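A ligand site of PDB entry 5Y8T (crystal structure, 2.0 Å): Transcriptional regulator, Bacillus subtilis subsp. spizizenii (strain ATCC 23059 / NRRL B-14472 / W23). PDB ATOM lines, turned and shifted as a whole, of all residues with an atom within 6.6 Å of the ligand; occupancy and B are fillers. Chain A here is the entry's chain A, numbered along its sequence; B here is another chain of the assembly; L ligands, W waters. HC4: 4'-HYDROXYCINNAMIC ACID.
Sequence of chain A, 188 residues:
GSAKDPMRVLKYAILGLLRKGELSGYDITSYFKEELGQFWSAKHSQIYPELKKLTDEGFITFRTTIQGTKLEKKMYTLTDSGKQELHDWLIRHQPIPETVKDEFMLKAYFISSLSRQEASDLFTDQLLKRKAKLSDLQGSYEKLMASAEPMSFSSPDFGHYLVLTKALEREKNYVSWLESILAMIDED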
ATOM      1  N   GLU A  34      32.015  -7.017  23.957  1.00  0.00           N
ATOM      2  CA  GLU A  34      30.602  -7.357  23.703  1.00  0.00           C
ATOM      3  C   GLU A  34      30.295  -8.765  24.241  1.00  0.00           C
ATOM      4  O   GLU A  34      30.629  -9.083  25.383  1.00  0.00           O
ATOM      5  CB  GLU A  34      30.266  -7.195  22.202  1.00  0.00           C
ATOM      6  N   GLU A  35      29.667  -9.596  23.397  1.00  0.00           N
ATOM      7  CA  GLU A  35      29.125 -10.906  23.799  1.00  0.00           C
ATOM      8  C   GLU A  35      30.198 -11.964  24.006  1.00  0.00           C
ATOM      9  O   GLU A  35      30.037 -12.869  24.816  1.00  0.00           O
ATOM     10  CB  GLU A  35      28.126 -11.402  22.739  1.00  0.00           C
ATOM     11  CG  GLU A  35      28.783 -11.798  21.444  1.00  0.00           C
ATOM     12  CD  GLU A  35      28.029 -11.404  20.208  1.00  0.00           C
ATOM     13  OE1 GLU A  35      27.528 -10.282  20.142  1.00  0.00           O
ATOM     14  OE2 GLU A  35      27.986 -12.236  19.272  1.00  0.00           O
ATOM     15  N   LEU A  36      31.280 -11.854  23.247  1.00  0.00           N
ATOM     16  CA  LEU A  36      32.391 -12.792  23.385  1.00  0.00           C
ATOM     17  C   LEU A  36      32.975 -12.695  24.792  1.00  0.00           C
ATOM     18  O   LEU A  36      33.297 -13.716  25.371  1.00  0.00           O
ATOM     19  CB  LEU A  36      33.475 -12.535  22.321  1.00  0.00           C
ATOM     20  CG  LEU A  36      34.697 -13.463  22.297  1.00  0.00           C
ATOM     21  CD1 LEU A  36      34.316 -14.933  22.269  1.00  0.00           C
ATOM     22  CD2 LEU A  36      35.624 -13.126  21.106  1.00  0.00           C
ATOM     23  N   GLN A  38      31.553 -12.077  27.673  1.00  0.00           N
ATOM     24  CA  GLN A  38      30.769 -12.640  28.764  1.00  0.00           C
ATOM     25  C   GLN A  38      31.215 -14.062  29.120  1.00  0.00           C
ATOM     26  O   GLN A  38      31.151 -14.454  30.268  1.00  0.00           O
ATOM     27  CB  GLN A  38      29.285 -12.616  28.398  1.00  0.00           C
ATOM     28  CG  GLN A  38      28.686 -11.222  28.309  1.00  0.00           C
ATOM     29  CD  GLN A  38      28.864 -10.443  29.581  1.00  0.00           C
ATOM     30  OE1 GLN A  38      28.152 -10.697  30.581  1.00  0.00           O
ATOM     31  NE2 GLN A  38      29.816  -9.484  29.552  1.00  0.00           N
ATOM     32  N   PHE A  39      31.691 -14.832  28.149  1.00  0.00           N
ATOM     33  CA  PHE A  39      32.017 -16.230  28.434  1.00  0.00           C
ATOM     34  C   PHE A  39      33.487 -16.541  28.111  1.00  0.00           C
ATOM     35  O   PHE A  39      33.987 -17.635  28.395  1.00  0.00           O
ATOM     36  CB  PHE A  39      31.059 -17.126  27.651  1.00  0.00           C
ATOM     37  CG  PHE A  39      31.243 -17.069  26.144  1.00  0.00           C
ATOM     38  CD1 PHE A  39      30.592 -16.108  25.382  1.00  0.00           C
ATOM     39  CD2 PHE A  39      32.069 -17.967  25.503  1.00  0.00           C
ATOM     40  CE1 PHE A  39      30.766 -16.046  24.016  1.00  0.00           C
ATOM     41  CE2 PHE A  39      32.250 -17.891  24.122  1.00  0.00           C
ATOM     42  CZ  PHE A  39      31.594 -16.919  23.394  1.00  0.00           C
ATOM     43  N   TRP A  40      34.180 -15.569  27.553  1.00  0.00           N
ATOM     44  CA  TRP A  40      35.600 -15.723  27.192  1.00  0.00           C
ATOM     45  C   TRP A  40      36.301 -14.377  27.310  1.00  0.00           C
ATOM     46  O   TRP A  40      36.801 -13.799  26.318  1.00  0.00           O
ATOM     47  CB  TRP A  40      35.759 -16.282  25.782  1.00  0.00           C
ATOM     48  CG  TRP A  40      37.047 -17.000  25.623  1.00  0.00           C
ATOM     49  CD1 TRP A  40      38.248 -16.455  25.278  1.00  0.00           C
ATOM     50  CD2 TRP A  40      37.296 -18.383  25.869  1.00  0.00           C
ATOM     51  NE1 TRP A  40      39.219 -17.420  25.248  1.00  0.00           N
ATOM     52  CE2 TRP A  40      38.664 -18.620  25.606  1.00  0.00           C
ATOM     53  CE3 TRP A  40      36.482 -19.464  26.221  1.00  0.00           C
ATOM     54  CZ2 TRP A  40      39.250 -19.879  25.719  1.00  0.00           C
ATOM     55  CZ3 TRP A  40      37.064 -20.716  26.340  1.00  0.00           C
ATOM     56  CH2 TRP A  40      38.439 -20.911  26.094  1.00  0.00           C
ATOM     57  N   LYS A 133      21.497 -12.474  37.721  1.00  0.00           N
ATOM     58  CA  LYS A 133      22.321 -12.760  36.550  1.00  0.00           C
ATOM     59  C   LYS A 133      21.419 -13.321  35.451  1.00  0.00           C
ATOM     60  O   LYS A 133      21.548 -12.959  34.271  1.00  0.00           O
ATOM     61  CB  LYS A 133      23.472 -13.730  36.919  1.00  0.00           C
ATOM     62  CG  LYS A 133      24.272 -14.217  35.671  1.00  0.00           C
ATOM     63  CD  LYS A 133      25.474 -15.061  36.071  1.00  0.00           C
ATOM     64  CE  LYS A 133      26.241 -15.543  34.820  1.00  0.00           C
ATOM     65  NZ  LYS A 133      26.383 -14.415  33.800  1.00  0.00           N
ATOM     66  N   ASP A 136      19.651 -10.593  33.605  1.00  0.00           N
ATOM     67  CA  ASP A 136      20.518  -9.917  32.630  1.00  0.00           C
ATOM     68  C   ASP A 136      20.625 -10.763  31.360  1.00  0.00           C
ATOM     69  O   ASP A 136      20.570 -10.243  30.263  1.00  0.00           O
ATOM     70  CB  ASP A 136      21.908  -9.625  33.189  1.00  0.00           C
ATOM     71  CG  ASP A 136      21.902  -8.540  34.252  1.00  0.00           C
ATOM     72  OD1 ASP A 136      21.017  -7.672  34.260  1.00  0.00           O
ATOM     73  OD2 ASP A 136      22.788  -8.599  35.122  1.00  0.00           O
ATOM     74  N   LEU A 137      20.791 -12.066  31.515  1.00  0.00           N
ATOM     75  CA  LEU A 137      20.847 -12.973  30.384  1.00  0.00           C
ATOM     76  C   LEU A 137      19.544 -12.971  29.574  1.00  0.00           C
ATOM     77  O   LEU A 137      19.581 -13.060  28.335  1.00  0.00           O
ATOM     78  CB  LEU A 137      21.200 -14.387  30.838  1.00  0.00           C
ATOM     79  CG  LEU A 137      22.608 -14.577  31.447  1.00  0.00           C
ATOM     80  CD1 LEU A 137      22.722 -16.035  32.097  1.00  0.00           C
ATOM     81  CD2 LEU A 137      23.711 -14.337  30.329  1.00  0.00           C
ATOM     82  N   SER A 140      19.478 -10.091  27.297  1.00  0.00           N
ATOM     83  CA  SER A 140      20.332 -10.342  26.147  1.00  0.00           C
ATOM     84  C   SER A 140      19.658 -11.259  25.138  1.00  0.00           C
ATOM     85  O   SER A 140      19.689 -10.984  23.937  1.00  0.00           O
ATOM     86  CB  SER A 140      21.659 -10.898  26.594  1.00  0.00           C
ATOM     87  OG  SER A 140      22.326  -9.916  27.365  1.00  0.00           O
ATOM     88  N   TYR A 141      18.991 -12.301  25.628  1.00  0.00           N
ATOM     89  CA  TYR A 141      18.230 -13.237  24.770  1.00  0.00           C
ATOM     90  C   TYR A 141      17.134 -12.520  23.974  1.00  0.00           C
ATOM     91  O   TYR A 141      16.988 -12.731  22.769  1.00  0.00           O
ATOM     92  CB  TYR A 141      17.610 -14.325  25.630  1.00  0.00           C
ATOM     93  CG  TYR A 141      16.917 -15.389  24.867  1.00  0.00           C
ATOM     94  CD1 TYR A 141      17.632 -16.402  24.252  1.00  0.00           C
ATOM     95  CD2 TYR A 141      15.536 -15.398  24.745  1.00  0.00           C
ATOM     96  CE1 TYR A 141      16.998 -17.399  23.551  1.00  0.00           C
ATOM     97  CE2 TYR A 141      14.885 -16.378  24.047  1.00  0.00           C
ATOM     98  CZ  TYR A 141      15.618 -17.383  23.447  1.00  0.00           C
ATOM     99  OH  TYR A 141      14.993 -18.373  22.725  1.00  0.00           O
ATOM    100  N   LEU A 144      18.681 -10.542  21.165  1.00  0.00           N
ATOM    101  CA  LEU A 144      19.087 -11.433  20.095  1.00  0.00           C
ATOM    102  C   LEU A 144      17.872 -11.900  19.318  1.00  0.00           C
ATOM    103  O   LEU A 144      17.894 -11.916  18.097  1.00  0.00           O
ATOM    104  CB  LEU A 144      19.846 -12.656  20.651  1.00  0.00           C
ATOM    105  CG  LEU A 144      20.200 -13.798  19.709  1.00  0.00           C
ATOM    106  CD1 LEU A 144      21.073 -13.250  18.629  1.00  0.00           C
ATOM    107  CD2 LEU A 144      20.866 -14.969  20.492  1.00  0.00           C
ATOM    108  N   HIS A 160      25.947 -17.342  18.588  1.00  0.00           N
ATOM    109  CA  HIS A 160      25.527 -16.479  19.703  1.00  0.00           C
ATOM    110  C   HIS A 160      24.358 -17.105  20.506  1.00  0.00           C
ATOM    111  O   HIS A 160      24.337 -17.098  21.756  1.00  0.00           O
ATOM    112  CB  HIS A 160      25.159 -15.120  19.076  1.00  0.00           C
ATOM    113  CG  HIS A 160      24.942 -14.017  20.065  1.00  0.00           C
ATOM    114  ND1 HIS A 160      24.908 -12.691  19.690  1.00  0.00           N
ATOM    115  CD2 HIS A 160      24.789 -14.044  21.415  1.00  0.00           C
ATOM    116  CE1 HIS A 160      24.706 -11.944  20.770  1.00  0.00           C
ATOM    117  NE2 HIS A 160      24.663 -12.734  21.828  1.00  0.00           N
ATOM    118  N   VAL A 163      25.784 -19.843  22.877  1.00  0.00           N
ATOM    119  CA  VAL A 163      26.426 -19.412  24.104  1.00  0.00           C
ATOM    120  C   VAL A 163      25.420 -18.761  25.059  1.00  0.00           C
ATOM    121  O   VAL A 163      25.510 -18.895  26.288  1.00  0.00           O
ATOM    122  CB  VAL A 163      27.627 -18.529  23.851  1.00  0.00           C
ATOM    123  CG1 VAL A 163      28.702 -19.267  23.108  1.00  0.00           C
ATOM    124  CG2 VAL A 163      27.248 -17.241  23.089  1.00  0.00           C
ATOM    125  N   LEU A 164      24.409 -18.089  24.513  1.00  0.00           N
ATOM    126  CA  LEU A 164      23.428 -17.435  25.392  1.00  0.00           C
ATOM    127  C   LEU A 164      22.440 -18.448  25.997  1.00  0.00           C
ATOM    128  O   LEU A 164      22.172 -18.387  27.195  1.00  0.00           O
ATOM    129  CB  LEU A 164      22.700 -16.338  24.641  1.00  0.00           C
ATOM    130  CG  LEU A 164      21.745 -15.446  25.362  1.00  0.00           C
ATOM    131  CD1 LEU A 164      22.304 -15.054  26.786  1.00  0.00           C
ATOM    132  CD2 LEU A 164      21.532 -14.211  24.408  1.00  0.00           C
ATOM    133  N   THR A 165      21.919 -19.393  25.215  1.00  0.00           N
ATOM    134  CA  THR A 165      21.057 -20.435  25.815  1.00  0.00           C
ATOM    135  C   THR A 165      21.836 -21.344  26.790  1.00  0.00           C
ATOM    136  O   THR A 165      21.275 -21.803  27.804  1.00  0.00           O
ATOM    137  CB  THR A 165      20.337 -21.332  24.741  1.00  0.00           C
ATOM    138  OG1 THR A 165      21.321 -21.935  23.899  1.00  0.00           O
ATOM    139  CG2 THR A 165      19.398 -20.502  23.874  1.00  0.00           C
ATOM    140  N   LYS A 166      23.099 -21.641  26.503  1.00  0.00           N
ATOM    141  CA  LYS A 166      23.909 -22.384  27.467  1.00  0.00           C
ATOM    142  C   LYS A 166      23.989 -21.637  28.783  1.00  0.00           C
ATOM    143  O   LYS A 166      23.805 -22.224  29.836  1.00  0.00           O
ATOM    144  CB  LYS A 166      25.325 -22.625  26.944  1.00  0.00           C
ATOM    145  CG  LYS A 166      26.206 -23.453  27.898  1.00  0.00           C
ATOM    146  CD  LYS A 166      25.736 -24.915  27.904  1.00  0.00           C
ATOM    147  CE  LYS A 166      26.527 -25.757  28.850  1.00  0.00           C
ATOM    148  NZ  LYS A 166      26.062 -25.512  30.227  1.00  0.00           N
ATOM    149  N   ALA A 167      24.239 -20.333  28.740  1.00  0.00           N
ATOM    150  CA  ALA A 167      24.336 -19.526  29.971  1.00  0.00           C
ATOM    151  C   ALA A 167      22.989 -19.429  30.677  1.00  0.00           C
ATOM    152  O   ALA A 167      22.904 -19.576  31.891  1.00  0.00           O
ATOM    153  CB  ALA A 167      24.922 -18.142  29.665  1.00  0.00           C
ATOM    154  N   ARG A 170      22.409 -22.837  32.341  1.00  0.00           N
ATOM    155  CA  ARG A 170      23.308 -22.983  33.481  1.00  0.00           C
ATOM    156  C   ARG A 170      22.822 -22.229  34.704  1.00  0.00           C
ATOM    157  O   ARG A 170      22.856 -22.775  35.773  1.00  0.00           O
ATOM    158  CB  ARG A 170      24.716 -22.489  33.113  1.00  0.00           C
ATOM    159  CG  ARG A 170      25.822 -22.699  34.146  1.00  0.00           C
ATOM    160  CD  ARG A 170      27.137 -22.016  33.594  1.00  0.00           C
ATOM    161  NE  ARG A 170      26.826 -20.587  33.615  1.00  0.00           N
ATOM    162  CZ  ARG A 170      27.205 -19.662  32.732  1.00  0.00           C
ATOM    163  NH1 ARG A 170      27.978 -19.947  31.720  1.00  0.00           N
ATOM    164  NH2 ARG A 170      26.761 -18.398  32.883  1.00  0.00           N
ATOM    165  N   GLU A 171      22.413 -20.956  34.557  1.00  0.00           N
ATOM    166  CA  GLU A 171      21.946 -20.179  35.692  1.00  0.00           C
ATOM    167  C   GLU A 171      20.566 -20.617  36.170  1.00  0.00           C
ATOM    168  O   GLU A 171      20.311 -20.631  37.386  1.00  0.00           O
ATOM    169  CB  GLU A 171      21.960 -18.682  35.357  1.00  0.00           C
ATOM    170  CG  GLU A 171      23.317 -18.164  35.003  1.00  0.00           C
ATOM    171  CD  GLU A 171      24.416 -18.450  36.045  1.00  0.00           C
ATOM    172  OE1 GLU A 171      24.096 -18.487  37.243  1.00  0.00           O
ATOM    173  OE2 GLU A 171      25.592 -18.595  35.657  1.00  0.00           O
ATOM    174  N   GLU B  98      33.159 -13.837  37.137  1.00  0.00           N
ATOM    175  CA  GLU B  98      33.131 -13.950  35.694  1.00  0.00           C
ATOM    176  C   GLU B  98      32.987 -15.403  35.301  1.00  0.00           C
ATOM    177  O   GLU B  98      33.469 -16.349  35.980  1.00  0.00           O
ATOM    178  CB  GLU B  98      34.387 -13.276  35.109  1.00  0.00           C
ATOM    179  CG  GLU B  98      35.184 -14.045  34.069  1.00  0.00           C
ATOM    180  CD  GLU B  98      36.573 -13.476  33.969  1.00  0.00           C
ATOM    181  OE1 GLU B  98      37.533 -14.165  34.412  1.00  0.00           O
ATOM    182  OE2 GLU B  98      36.682 -12.313  33.515  1.00  0.00           O
ATOM    183  N   THR B  99      32.286 -15.583  34.216  1.00  0.00           N
ATOM    184  CA  THR B  99      32.004 -16.922  33.730  1.00  0.00           C
ATOM    185  C   THR B  99      33.260 -17.749  33.474  1.00  0.00           C
ATOM    186  O   THR B  99      34.256 -17.217  32.896  1.00  0.00           O
ATOM    187  CB  THR B  99      31.148 -16.820  32.464  1.00  0.00           C
ATOM    188  OG1 THR B  99      29.884 -16.251  32.859  1.00  0.00           O
ATOM    189  CG2 THR B  99      31.007 -18.188  31.709  1.00  0.00           C
ATOM    190  N   VAL B 100      33.204 -19.032  33.871  1.00  0.00           N
ATOM    191  CA  VAL B 100      34.340 -19.979  33.625  1.00  0.00           C
ATOM    192  C   VAL B 100      34.425 -20.305  32.172  1.00  0.00           C
ATOM    193  O   VAL B 100      33.401 -20.611  31.550  1.00  0.00           O
ATOM    194  CB  VAL B 100      34.169 -21.347  34.329  1.00  0.00           C
ATOM    195  N   TYR B 109      30.399 -21.205  19.830  1.00  0.00           N
ATOM    196  CA  TYR B 109      30.298 -19.814  19.339  1.00  0.00           C
ATOM    197  C   TYR B 109      30.738 -19.646  17.879  1.00  0.00           C
ATOM    198  O   TYR B 109      30.176 -18.832  17.145  1.00  0.00           O
ATOM    199  CB  TYR B 109      31.124 -18.920  20.231  1.00  0.00           C
ATOM    200  CG  TYR B 109      30.949 -17.442  19.965  1.00  0.00           C
ATOM    201  CD1 TYR B 109      29.731 -16.813  20.171  1.00  0.00           C
ATOM    202  CD2 TYR B 109      32.001 -16.685  19.550  1.00  0.00           C
ATOM    203  CE1 TYR B 109      29.563 -15.425  19.940  1.00  0.00           C
ATOM    204  CE2 TYR B 109      31.862 -15.319  19.310  1.00  0.00           C
ATOM    205  CZ  TYR B 109      30.641 -14.689  19.530  1.00  0.00           C
ATOM    206  OH  TYR B 109      30.518 -13.371  19.290  1.00  0.00           O
HETATM  207  C1  HC4 L   1      27.766 -16.185  30.276  1.00  0.00           C
HETATM  208  O1  HC4 L   1      27.676 -15.902  31.513  1.00  0.00           O
HETATM  209  O2  HC4 L   1      28.289 -17.218  29.816  1.00  0.00           O
HETATM  210  C2  HC4 L   1      27.145 -15.227  29.381  1.00  0.00           C
HETATM  211  C3  HC4 L   1      27.036 -15.441  28.080  1.00  0.00           C
HETATM  212  C1' HC4 L   1      26.385 -14.455  27.186  1.00  0.00           C
HETATM  213  C2' HC4 L   1      26.381 -14.787  25.831  1.00  0.00           C
HETATM  214  C3' HC4 L   1      25.820 -13.939  24.885  1.00  0.00           C
HETATM  215  C4' HC4 L   1      25.225 -12.736  25.280  1.00  0.00           C
HETATM  216  C5' HC4 L   1      25.218 -12.377  26.644  1.00  0.00           C
HETATM  217  C6' HC4 L   1      25.794 -13.241  27.601  1.00  0.00           C
HETATM  218  O4' HC4 L   1      24.664 -11.951  24.314  1.00  0.00           O
HETATM  219  O   HOH W   1      28.046 -19.529  27.597  1.00  0.00           O
HETATM  220  O   HOH W   2      28.120 -13.518  31.823  1.00  0.00           O
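Residues that only touch the ligand: Glu 35 (3.8 Å), Gln 38 (3.5 Å), Phe 39 (3.5 Å), Leu 137 (3.6 Å), Ser 140 (3.9 Å), Val 163 (3.8 Å), Leu 164 (3.9 Å) and Ala 167 (3.5 Å). Within 4 Å of the ligand: Glu 35, Gln 38, Phe 39, Lys 133, Leu 137, Ser 140, His 160, Val 163, Leu 164, Ala 167, Arg 170 and Thr 99 of chain B. Along chain A the residues within 4 Å of the ligand span positions 35 to 170.
Water W2 lies within hydrogen-bond range of O1 of the ligand (2.4 Å), NZ of Lys 133 (2.8 Å), OE1 of Gln 38 (3.1 Å) and OG1 of Thr 99 of chain B (3.4 Å). Water W1 bridges O of Val 163 (2.9 Å) and O2 of the ligand (3.2 Å).
A ring nitrogen (ND1) of His 160 lies within hydrogen-bond range of the side-chain carboxylate of Glu 35. The side-chain hydroxyl (OG1) of Thr 99 of chain B lies close to the backbone carbonyl oxygen (O) of Gln 38 (3.4 Å). The guanidinium group (NH2) of Arg 170 is in salt-bridge range of the side-chain carboxylate (OE2) of Glu 171 (3.0 Å). OH of Tyr 109 of chain B is in hydrogen-bond range of OE2 of Glu 35 (2.8 Å). The side-chain hydroxyl (OG) of Ser 140 is in hydrogen-bond range of the backbone carbonyl oxygen (O) of Asp 136.
O4' of the ligand sits at hydrogen-bond distance from NE2 of His 160 (2.6 Å). The side-chain hydroxyl (OG1) of Thr 99 of chain B sits at hydrogen-bond distance from an oxygen (O1) of the ligand (2.6 Å). An oxygen (O1) of the ligand is in salt-bridge range of the guanidinium group of Arg 170 (3.0 Å). The side-chain amino group (NZ) of Lys 133 lies within salt-bridge range of an oxygen (O1) of the ligand, 3.0 Å away.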
